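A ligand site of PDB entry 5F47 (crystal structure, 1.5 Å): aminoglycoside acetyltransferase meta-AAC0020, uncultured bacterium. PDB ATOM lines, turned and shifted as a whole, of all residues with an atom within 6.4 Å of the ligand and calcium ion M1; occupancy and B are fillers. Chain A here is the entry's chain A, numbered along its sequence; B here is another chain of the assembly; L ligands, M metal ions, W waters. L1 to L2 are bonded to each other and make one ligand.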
ATOM      1  N   VAL A  34     -13.340 -30.542   2.009  1.00  0.00           N
ATOM      2  CA  VAL A  34     -14.557 -31.194   2.464  1.00  0.00           C
ATOM      3  C   VAL A  34     -15.556 -30.164   2.970  1.00  0.00           C
ATOM      4  O   VAL A  34     -16.766 -30.281   2.694  1.00  0.00           O
ATOM      5  CB  VAL A  34     -14.243 -32.244   3.545  1.00  0.00           C
ATOM      6  CG1 VAL A  34     -15.528 -32.814   4.139  1.00  0.00           C
ATOM      7  CG2 VAL A  34     -13.398 -33.361   2.942  1.00  0.00           C
ATOM      8  N   PHE A  35     -15.085 -29.150   3.686  1.00  0.00           N
ATOM      9  CA  PHE A  35     -15.985 -28.127   4.209  1.00  0.00           C
ATOM     10  C   PHE A  35     -16.325 -27.075   3.153  1.00  0.00           C
ATOM     11  O   PHE A  35     -17.137 -26.182   3.402  1.00  0.00           O
ATOM     12  CB  PHE A  35     -15.394 -27.450   5.464  1.00  0.00           C
ATOM     13  CG  PHE A  35     -15.064 -28.405   6.594  1.00  0.00           C
ATOM     14  CD1 PHE A  35     -15.809 -29.568   6.775  1.00  0.00           C
ATOM     15  CD2 PHE A  35     -14.016 -28.143   7.471  1.00  0.00           C
ATOM     16  CE1 PHE A  35     -15.477 -30.454   7.809  1.00  0.00           C
ATOM     17  CE2 PHE A  35     -13.698 -29.028   8.511  1.00  0.00           C
ATOM     18  CZ  PHE A  35     -14.434 -30.168   8.673  1.00  0.00           C
ATOM     19  N   GLU A  36     -15.694 -27.177   1.982  1.00  0.00           N
ATOM     20  CA  GLU A  36     -15.934 -26.240   0.881  1.00  0.00           C
ATOM     21  C   GLU A  36     -15.716 -24.795   1.328  1.00  0.00           C
ATOM     22  O   GLU A  36     -16.528 -23.908   1.050  1.00  0.00           O
ATOM     23  CB  GLU A  36     -17.353 -26.426   0.318  1.00  0.00           C
ATOM     24  CG  GLU A  36     -17.612 -27.819  -0.244  1.00  0.00           C
ATOM     25  CD  GLU A  36     -19.061 -28.015  -0.668  1.00  0.00           C
ATOM     26  OE1 GLU A  36     -19.294 -28.416  -1.832  1.00  0.00           O
ATOM     27  OE2 GLU A  36     -19.969 -27.777   0.162  1.00  0.00           O
ATOM     28  N   MET A  37     -14.599 -24.560   2.005  1.00  0.00           N
ATOM     29  CA  MET A  37     -14.247 -23.219   2.460  1.00  0.00           C
ATOM     30  C   MET A  37     -13.908 -22.311   1.281  1.00  0.00           C
ATOM     31  O   MET A  37     -13.183 -22.707   0.362  1.00  0.00           O
ATOM     32  CB  MET A  37     -13.072 -23.300   3.435  1.00  0.00           C
ATOM     33  CG  MET A  37     -13.390 -24.139   4.676  1.00  0.00           C
ATOM     34  SD  MET A  37     -11.986 -24.256   5.800  1.00  0.00           S
ATOM     35  CE  MET A  37     -11.779 -22.555   6.285  1.00  0.00           C
ATOM     36  N   TYR A  88     -11.756 -31.324  23.580  1.00  0.00           N
ATOM     37  CA  TYR A  88     -12.728 -30.708  22.691  1.00  0.00           C
ATOM     38  C   TYR A  88     -12.339 -31.045  21.250  1.00  0.00           C
ATOM     39  O   TYR A  88     -11.345 -30.519  20.746  1.00  0.00           O
ATOM     40  CB  TYR A  88     -12.739 -29.199  22.932  1.00  0.00           C
ATOM     41  CG  TYR A  88     -13.669 -28.313  22.109  1.00  0.00           C
ATOM     42  CD1 TYR A  88     -14.721 -28.821  21.377  1.00  0.00           C
ATOM     43  CD2 TYR A  88     -13.454 -26.946  22.090  1.00  0.00           C
ATOM     44  CE1 TYR A  88     -15.557 -27.975  20.633  1.00  0.00           C
ATOM     45  CE2 TYR A  88     -14.276 -26.098  21.375  1.00  0.00           C
ATOM     46  CZ  TYR A  88     -15.310 -26.615  20.652  1.00  0.00           C
ATOM     47  OH  TYR A  88     -16.109 -25.757  19.933  1.00  0.00           O
ATOM     48  N   ILE A  89     -13.089 -31.941  20.631  1.00  0.00           N
ATOM     49  CA  ILE A  89     -12.904 -32.218  19.208  1.00  0.00           C
ATOM     50  C   ILE A  89     -13.444 -31.039  18.422  1.00  0.00           C
ATOM     51  O   ILE A  89     -14.632 -30.680  18.546  1.00  0.00           O
ATOM     52  CB  ILE A  89     -13.621 -33.508  18.782  1.00  0.00           C
ATOM     53  CG1 ILE A  89     -13.015 -34.738  19.501  1.00  0.00           C
ATOM     54  CG2 ILE A  89     -13.528 -33.627  17.243  1.00  0.00           C
ATOM     55  CD1 ILE A  89     -13.854 -35.997  19.314  1.00  0.00           C
ATOM     56  N   TYR A  90     -12.580 -30.393  17.626  1.00  0.00           N
ATOM     57  CA  TYR A  90     -12.947 -29.167  16.952  1.00  0.00           C
ATOM     58  C   TYR A  90     -13.404 -29.402  15.516  1.00  0.00           C
ATOM     59  O   TYR A  90     -14.436 -28.864  15.109  1.00  0.00           O
ATOM     60  CB  TYR A  90     -11.777 -28.163  16.999  1.00  0.00           C
ATOM     61  CG  TYR A  90     -12.252 -26.800  16.618  1.00  0.00           C
ATOM     62  CD1 TYR A  90     -12.905 -26.000  17.555  1.00  0.00           C
ATOM     63  CD2 TYR A  90     -12.125 -26.335  15.314  1.00  0.00           C
ATOM     64  CE1 TYR A  90     -13.396 -24.741  17.197  1.00  0.00           C
ATOM     65  CE2 TYR A  90     -12.611 -25.071  14.950  1.00  0.00           C
ATOM     66  CZ  TYR A  90     -13.234 -24.294  15.923  1.00  0.00           C
ATOM     67  OH  TYR A  90     -13.730 -23.070  15.578  1.00  0.00           O
ATOM     68  N   ASP A  91     -12.652 -30.172  14.755  1.00  0.00           N
ATOM     69  CA  ASP A  91     -13.040 -30.548  13.398  1.00  0.00           C
ATOM     70  C   ASP A  91     -12.830 -32.032  13.178  1.00  0.00           C
ATOM     71  O   ASP A  91     -11.931 -32.614  13.748  1.00  0.00           O
ATOM     72  CB  ASP A  91     -12.216 -29.813  12.346  1.00  0.00           C
ATOM     73  CG  ASP A  91     -12.748 -28.450  11.995  1.00  0.00           C
ATOM     74  OD1 ASP A  91     -13.966 -28.275  11.824  1.00  0.00           O
ATOM     75  OD2 ASP A  91     -11.905 -27.534  11.842  1.00  0.00           O
ATOM     76  N   LEU A  92     -13.692 -32.635  12.354  1.00  0.00           N
ATOM     77  CA  LEU A  92     -13.514 -34.006  11.886  1.00  0.00           C
ATOM     78  C   LEU A  92     -13.975 -34.054  10.437  1.00  0.00           C
ATOM     79  O   LEU A  92     -15.057 -33.537  10.094  1.00  0.00           O
ATOM     80  CB  LEU A  92     -14.312 -34.991  12.746  1.00  0.00           C
ATOM     81  CG  LEU A  92     -14.464 -36.442  12.241  1.00  0.00           C
ATOM     82  CD1 LEU A  92     -13.139 -37.214  12.113  1.00  0.00           C
ATOM     83  CD2 LEU A  92     -15.414 -37.218  13.165  1.00  0.00           C
ATOM     84  N   ALA A  93     -13.164 -34.650   9.561  1.00  0.00           N
ATOM     85  CA  ALA A  93     -13.546 -34.816   8.171  1.00  0.00           C
ATOM     86  C   ALA A  93     -12.897 -36.041   7.557  1.00  0.00           C
ATOM     87  O   ALA A  93     -11.814 -36.451   7.961  1.00  0.00           O
ATOM     88  CB  ALA A  93     -13.189 -33.568   7.350  1.00  0.00           C
ATOM     89  N   GLN A 126     -19.128 -30.847  18.665  1.00  0.00           N
ATOM     90  CA  GLN A 126     -20.314 -30.092  18.265  1.00  0.00           C
ATOM     91  C   GLN A 126     -20.721 -30.392  16.818  1.00  0.00           C
ATOM     92  O   GLN A 126     -19.857 -30.458  15.941  1.00  0.00           O
ATOM     93  CB  GLN A 126     -20.058 -28.595  18.427  1.00  0.00           C
ATOM     94  CG  GLN A 126     -21.227 -27.673  18.029  1.00  0.00           C
ATOM     95  CD  GLN A 126     -20.984 -26.234  18.428  1.00  0.00           C
ATOM     96  OE1 GLN A 126     -20.923 -25.900  19.608  1.00  0.00           O
ATOM     97  NE2 GLN A 126     -20.848 -25.356  17.427  1.00  0.00           N
ATOM     98  N   ALA A 127     -22.013 -30.552  16.560  1.00  0.00           N
ATOM     99  CA  ALA A 127     -22.507 -30.689  15.210  1.00  0.00           C
ATOM    100  C   ALA A 127     -23.707 -29.774  15.002  1.00  0.00           C
ATOM    101  O   ALA A 127     -24.442 -29.460  15.951  1.00  0.00           O
ATOM    102  CB  ALA A 127     -22.886 -32.151  14.911  1.00  0.00           C
ATOM    103  N   ASP A 128     -23.899 -29.325  13.771  1.00  0.00           N
ATOM    104  CA  ASP A 128     -25.012 -28.424  13.499  1.00  0.00           C
ATOM    105  C   ASP A 128     -26.298 -29.214  13.443  1.00  0.00           C
ATOM    106  O   ASP A 128     -26.342 -30.302  12.873  1.00  0.00           O
ATOM    107  CB  ASP A 128     -24.783 -27.641  12.211  1.00  0.00           C
ATOM    108  CG  ASP A 128     -25.744 -26.492  12.079  1.00  0.00           C
ATOM    109  OD1 ASP A 128     -25.370 -25.354  12.457  1.00  0.00           O
ATOM    110  OD2 ASP A 128     -26.890 -26.713  11.642  1.00  0.00           O
ATOM    111  N   ASP A 131     -27.420 -30.546  10.072  1.00  0.00           N
ATOM    112  CA  ASP A 131     -26.543 -31.512   9.422  1.00  0.00           C
ATOM    113  C   ASP A 131     -26.926 -32.932   9.835  1.00  0.00           C
ATOM    114  O   ASP A 131     -26.231 -33.543  10.646  1.00  0.00           O
ATOM    115  CB  ASP A 131     -25.089 -31.227   9.800  1.00  0.00           C
ATOM    116  CG  ASP A 131     -24.101 -31.901   8.867  1.00  0.00           C
ATOM    117  OD1 ASP A 131     -24.497 -32.835   8.126  1.00  0.00           O
ATOM    118  OD2 ASP A 131     -22.923 -31.492   8.910  1.00  0.00           O
ATOM    119  N   ALA A 134     -24.146 -35.589   9.800  1.00  0.00           N
ATOM    120  CA  ALA A 134     -23.190 -35.486  10.903  1.00  0.00           C
ATOM    121  C   ALA A 134     -23.812 -36.061  12.175  1.00  0.00           C
ATOM    122  O   ALA A 134     -23.165 -36.786  12.941  1.00  0.00           O
ATOM    123  CB  ALA A 134     -22.759 -34.032  11.129  1.00  0.00           C
ATOM    124  N   HIS A 151     -25.270 -22.090  20.097  1.00  0.00           N
ATOM    125  CA  HIS A 151     -23.911 -21.573  19.964  1.00  0.00           C
ATOM    126  C   HIS A 151     -23.994 -20.098  19.528  1.00  0.00           C
ATOM    127  O   HIS A 151     -24.622 -19.766  18.533  1.00  0.00           O
ATOM    128  CB  HIS A 151     -23.152 -22.440  18.950  1.00  0.00           C
ATOM    129  CG  HIS A 151     -21.827 -21.890  18.516  1.00  0.00           C
ATOM    130  ND1 HIS A 151     -20.651 -22.197  19.168  1.00  0.00           N
ATOM    131  CD2 HIS A 151     -21.494 -21.127  17.458  1.00  0.00           C
ATOM    132  CE1 HIS A 151     -19.645 -21.607  18.540  1.00  0.00           C
ATOM    133  NE2 HIS A 151     -20.128 -20.958  17.503  1.00  0.00           N
ATOM    134  N   TYR B  81      -6.922 -22.117  10.852  1.00  0.00           N
ATOM    135  CA  TYR B  81      -7.545 -21.405   9.732  1.00  0.00           C
ATOM    136  C   TYR B  81      -7.132 -19.931   9.645  1.00  0.00           C
ATOM    137  O   TYR B  81      -7.365 -19.291   8.625  1.00  0.00           O
ATOM    138  CB  TYR B  81      -9.077 -21.462   9.847  1.00  0.00           C
ATOM    139  CG  TYR B  81      -9.696 -22.850   9.689  1.00  0.00           C
ATOM    140  CD1 TYR B  81      -9.325 -23.684   8.638  1.00  0.00           C
ATOM    141  CD2 TYR B  81     -10.624 -23.308  10.608  1.00  0.00           C
ATOM    142  CE1 TYR B  81      -9.897 -24.944   8.505  1.00  0.00           C
ATOM    143  CE2 TYR B  81     -11.210 -24.556  10.474  1.00  0.00           C
ATOM    144  CZ  TYR B  81     -10.845 -25.365   9.424  1.00  0.00           C
ATOM    145  OH  TYR B  81     -11.409 -26.620   9.270  1.00  0.00           O
ATOM    146  N   GLU B 147     -26.396 -20.125  16.455  1.00  0.00           N
ATOM    147  CA  GLU B 147     -26.523 -21.360  15.685  1.00  0.00           C
ATOM    148  C   GLU B 147     -27.118 -22.464  16.553  1.00  0.00           C
ATOM    149  O   GLU B 147     -26.700 -22.645  17.703  1.00  0.00           O
ATOM    150  CB  GLU B 147     -25.163 -21.799  15.134  1.00  0.00           C
ATOM    151  CG  GLU B 147     -24.541 -20.742  14.218  1.00  0.00           C
ATOM    152  CD  GLU B 147     -23.179 -21.121  13.641  1.00  0.00           C
ATOM    153  OE1 GLU B 147     -22.537 -22.059  14.156  1.00  0.00           O
ATOM    154  OE2 GLU B 147     -22.769 -20.477  12.642  1.00  0.00           O
ATOM    155  N   VAL B 149     -27.220 -26.122  17.573  1.00  0.00           N
ATOM    156  CA  VAL B 149     -26.260 -27.199  17.467  1.00  0.00           C
ATOM    157  C   VAL B 149     -26.557 -28.295  18.471  1.00  0.00           C
ATOM    158  O   VAL B 149     -27.488 -28.187  19.279  1.00  0.00           O
ATOM    159  CB  VAL B 149     -24.802 -26.700  17.656  1.00  0.00           C
ATOM    160  CG1 VAL B 149     -24.462 -25.635  16.597  1.00  0.00           C
ATOM    161  CG2 VAL B 149     -24.595 -26.133  19.052  1.00  0.00           C
HETATM  162  C1  LIG L   1     -17.727 -28.068  10.467  1.00  0.00           C
HETATM  163  C2  LIG L   1     -17.503 -27.151   9.291  1.00  0.00           C
HETATM  164  C3  LIG L   1     -18.761 -27.017   8.481  1.00  0.00           C
HETATM  165  C4  LIG L   1     -19.184 -28.334   7.970  1.00  0.00           C
HETATM  166  C5  LIG L   1     -19.448 -29.251   9.141  1.00  0.00           C
HETATM  167  C6  LIG L   1     -19.855 -30.621   8.693  1.00  0.00           C
HETATM  168  O1  LIG L   1     -17.073 -25.870   9.809  1.00  0.00           O
HETATM  169  O2  LIG L   1     -18.545 -26.119   7.361  1.00  0.00           O
HETATM  170  O3  LIG L   1     -20.391 -28.189   7.165  1.00  0.00           O
HETATM  171  O4  LIG L   1     -18.237 -29.376   9.983  1.00  0.00           O
HETATM  172  O5  LIG L   1     -18.825 -31.264   7.965  1.00  0.00           O
HETATM  173  C1  LG2 L   2     -18.703 -28.129  12.622  1.00  0.00           C
HETATM  174  C2  LG2 L   2     -19.906 -27.683  13.409  1.00  0.00           C
HETATM  175  C3  LG2 L   2     -19.787 -26.242  13.846  1.00  0.00           C
HETATM  176  C4  LG2 L   2     -18.485 -25.925  14.516  1.00  0.00           C
HETATM  177  C5  LG2 L   2     -17.328 -26.353  13.625  1.00  0.00           C
HETATM  178  C6  LG2 L   2     -15.987 -26.131  14.231  1.00  0.00           C
HETATM  179  O1  LG2 L   2     -18.680 -27.479  11.357  1.00  0.00           O
HETATM  180  O2  LG2 L   2     -21.064 -27.840  12.575  1.00  0.00           O
HETATM  181  O3  LG2 L   2     -20.910 -25.939  14.735  1.00  0.00           O
HETATM  182  O4  LG2 L   2     -18.364 -24.506  14.824  1.00  0.00           O
HETATM  183  O5  LG2 L   2     -17.433 -27.799  13.339  1.00  0.00           O
HETATM  184  O6  LG2 L   2     -15.868 -26.772  15.532  1.00  0.00           O
HETATM  185 CA    CA M   1     -20.753 -28.676   4.803  1.00  0.00          CA
HETATM  186 CA    CA M   2     -18.760 -21.873  11.348  1.00  0.00          CA
HETATM  187  O   HOH W   1     -19.296 -26.837   4.986  1.00  0.00           O
HETATM  188  O   HOH W   2     -19.278 -28.963   2.840  1.00  0.00           O
HETATM  189  O   HOH W   3     -22.026 -30.307  11.754  1.00  0.00           O
HETATM  190  O   HOH W   4     -17.324 -30.073  15.095  1.00  0.00           O
HETATM  191  O   HOH W   5     -21.523 -25.630  10.889  1.00  0.00           O
HETATM  192  O   HOH W   6     -20.306 -23.672   7.602  1.00  0.00           O
HETATM  193  O   HOH W   7     -15.940 -30.768  11.782  1.00  0.00           O
HETATM  194  O   HOH W   8     -17.868 -24.029  17.277  1.00  0.00           O
HETATM  195  O   HOH W   9     -20.817 -33.748   7.694  1.00  0.00           O
HETATM  196  O   HOH W  10     -14.616 -25.770  10.814  1.00  0.00           O
HETATM  197  O   HOH W  11     -17.527 -32.176  10.204  1.00  0.00           O
HETATM  198  O   HOH W  12     -17.051 -22.824  12.944  1.00  0.00           O
HETATM  199  O   HOH W  13     -21.806 -27.913   2.789  1.00  0.00           O
HETATM  200  O   HOH W  14     -19.224 -24.140  10.735  1.00  0.00           O
HETATM  201  O   HOH W  15     -22.967 -24.722  13.244  1.00  0.00           O
HETATM  202  O   HOH W  16     -17.128 -33.764   8.191  1.00  0.00           O
HETATM  203  O   HOH W  17     -16.976 -22.413   9.875  1.00  0.00           O
HETATM  204  O   HOH W  18     -19.193 -30.520   5.371  1.00  0.00           O
HETATM  205  O   HOH W  19     -19.970 -22.497  13.476  1.00  0.00           O
HETATM  206  O   HOH W  20     -16.466 -24.140   7.284  1.00  0.00           O
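The backbone NH of Asp 128 lies within hydrogen-bond range of an oxygen (O2) of LG2 L2 (3.4 Å).
An oxygen (O6) of LG2 L2 is in hydrogen-bond range of the backbone carbonyl oxygen of Tyr 90 (2.6 Å).
An oxygen (O3) of LG2 L2 is in hydrogen-bond range of the side-chain amide nitrogen (NE2) of Gln 126.
No residue comes within 4 Å of calcium ion M1.
The nearest printed residue that does not touch calcium ion M1 is Phe 35 (4.6 Å).
The side-chain hydroxyl (OH) of Tyr 81 of chain B is in hydrogen-bond range of the side-chain carboxylate (OD2) of Asp 91 (2.8 Å).
OD1 of Asp 131 sits at hydrogen-bond distance from N of Ala 134.
Water W1 lies within hydrogen-bond range of O2 of LIG L1 and O of Phe 35.
Water W8 bridges O4 of LG2 L2 (2.5 Å) and NE2 of Gln 126 (3.3 Å).
Water W11 bridges O5 of LIG L1 (2.7 Å) and O of Leu 92 (2.8 Å).
Water W3 lies within hydrogen-bond range of O2 of LG2 L2 (2.8 Å), N of Asp 128 (2.9 Å) and OD2 of Asp 131 (3.2 Å).
Water W15 lies within hydrogen-bond range of the side-chain carboxylate (OD1) of Asp 128 (2.6 Å), an oxygen (O3) of LG2 L2 (2.8 Å) and the side-chain carboxylate (OE1) of Glu 147 of chain B (2.8 Å).
Water W16 lies within hydrogen-bond range of O of Leu 92 (2.8 Å) and O5 of LIG L1 (3.0 Å).
CE1 of Phe 35 touches O5 of LIG L1, 3.4 Å away.
OD1 of Asp 91 touches C6 of LG2 L2, 3.8 Å away.
OD2 of Asp 131 touches C6 of LIG L1, 3.2 Å away.
Of the 19 residues printed, 6 come within 4 Å of the ligand.
Water W1 binds calcium ion M1.
Calcium ion M1 is bound by water W13 (2.4 Å).
Calcium ion M1 is bound by an oxygen (O3) of LIG L1, 2.4 Å away.
Water W2 binds calcium ion M1 (2.5 Å).
Water W18 is bound to calcium ion M1.
Calcium ion M1 has five donor atoms within binding distance.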
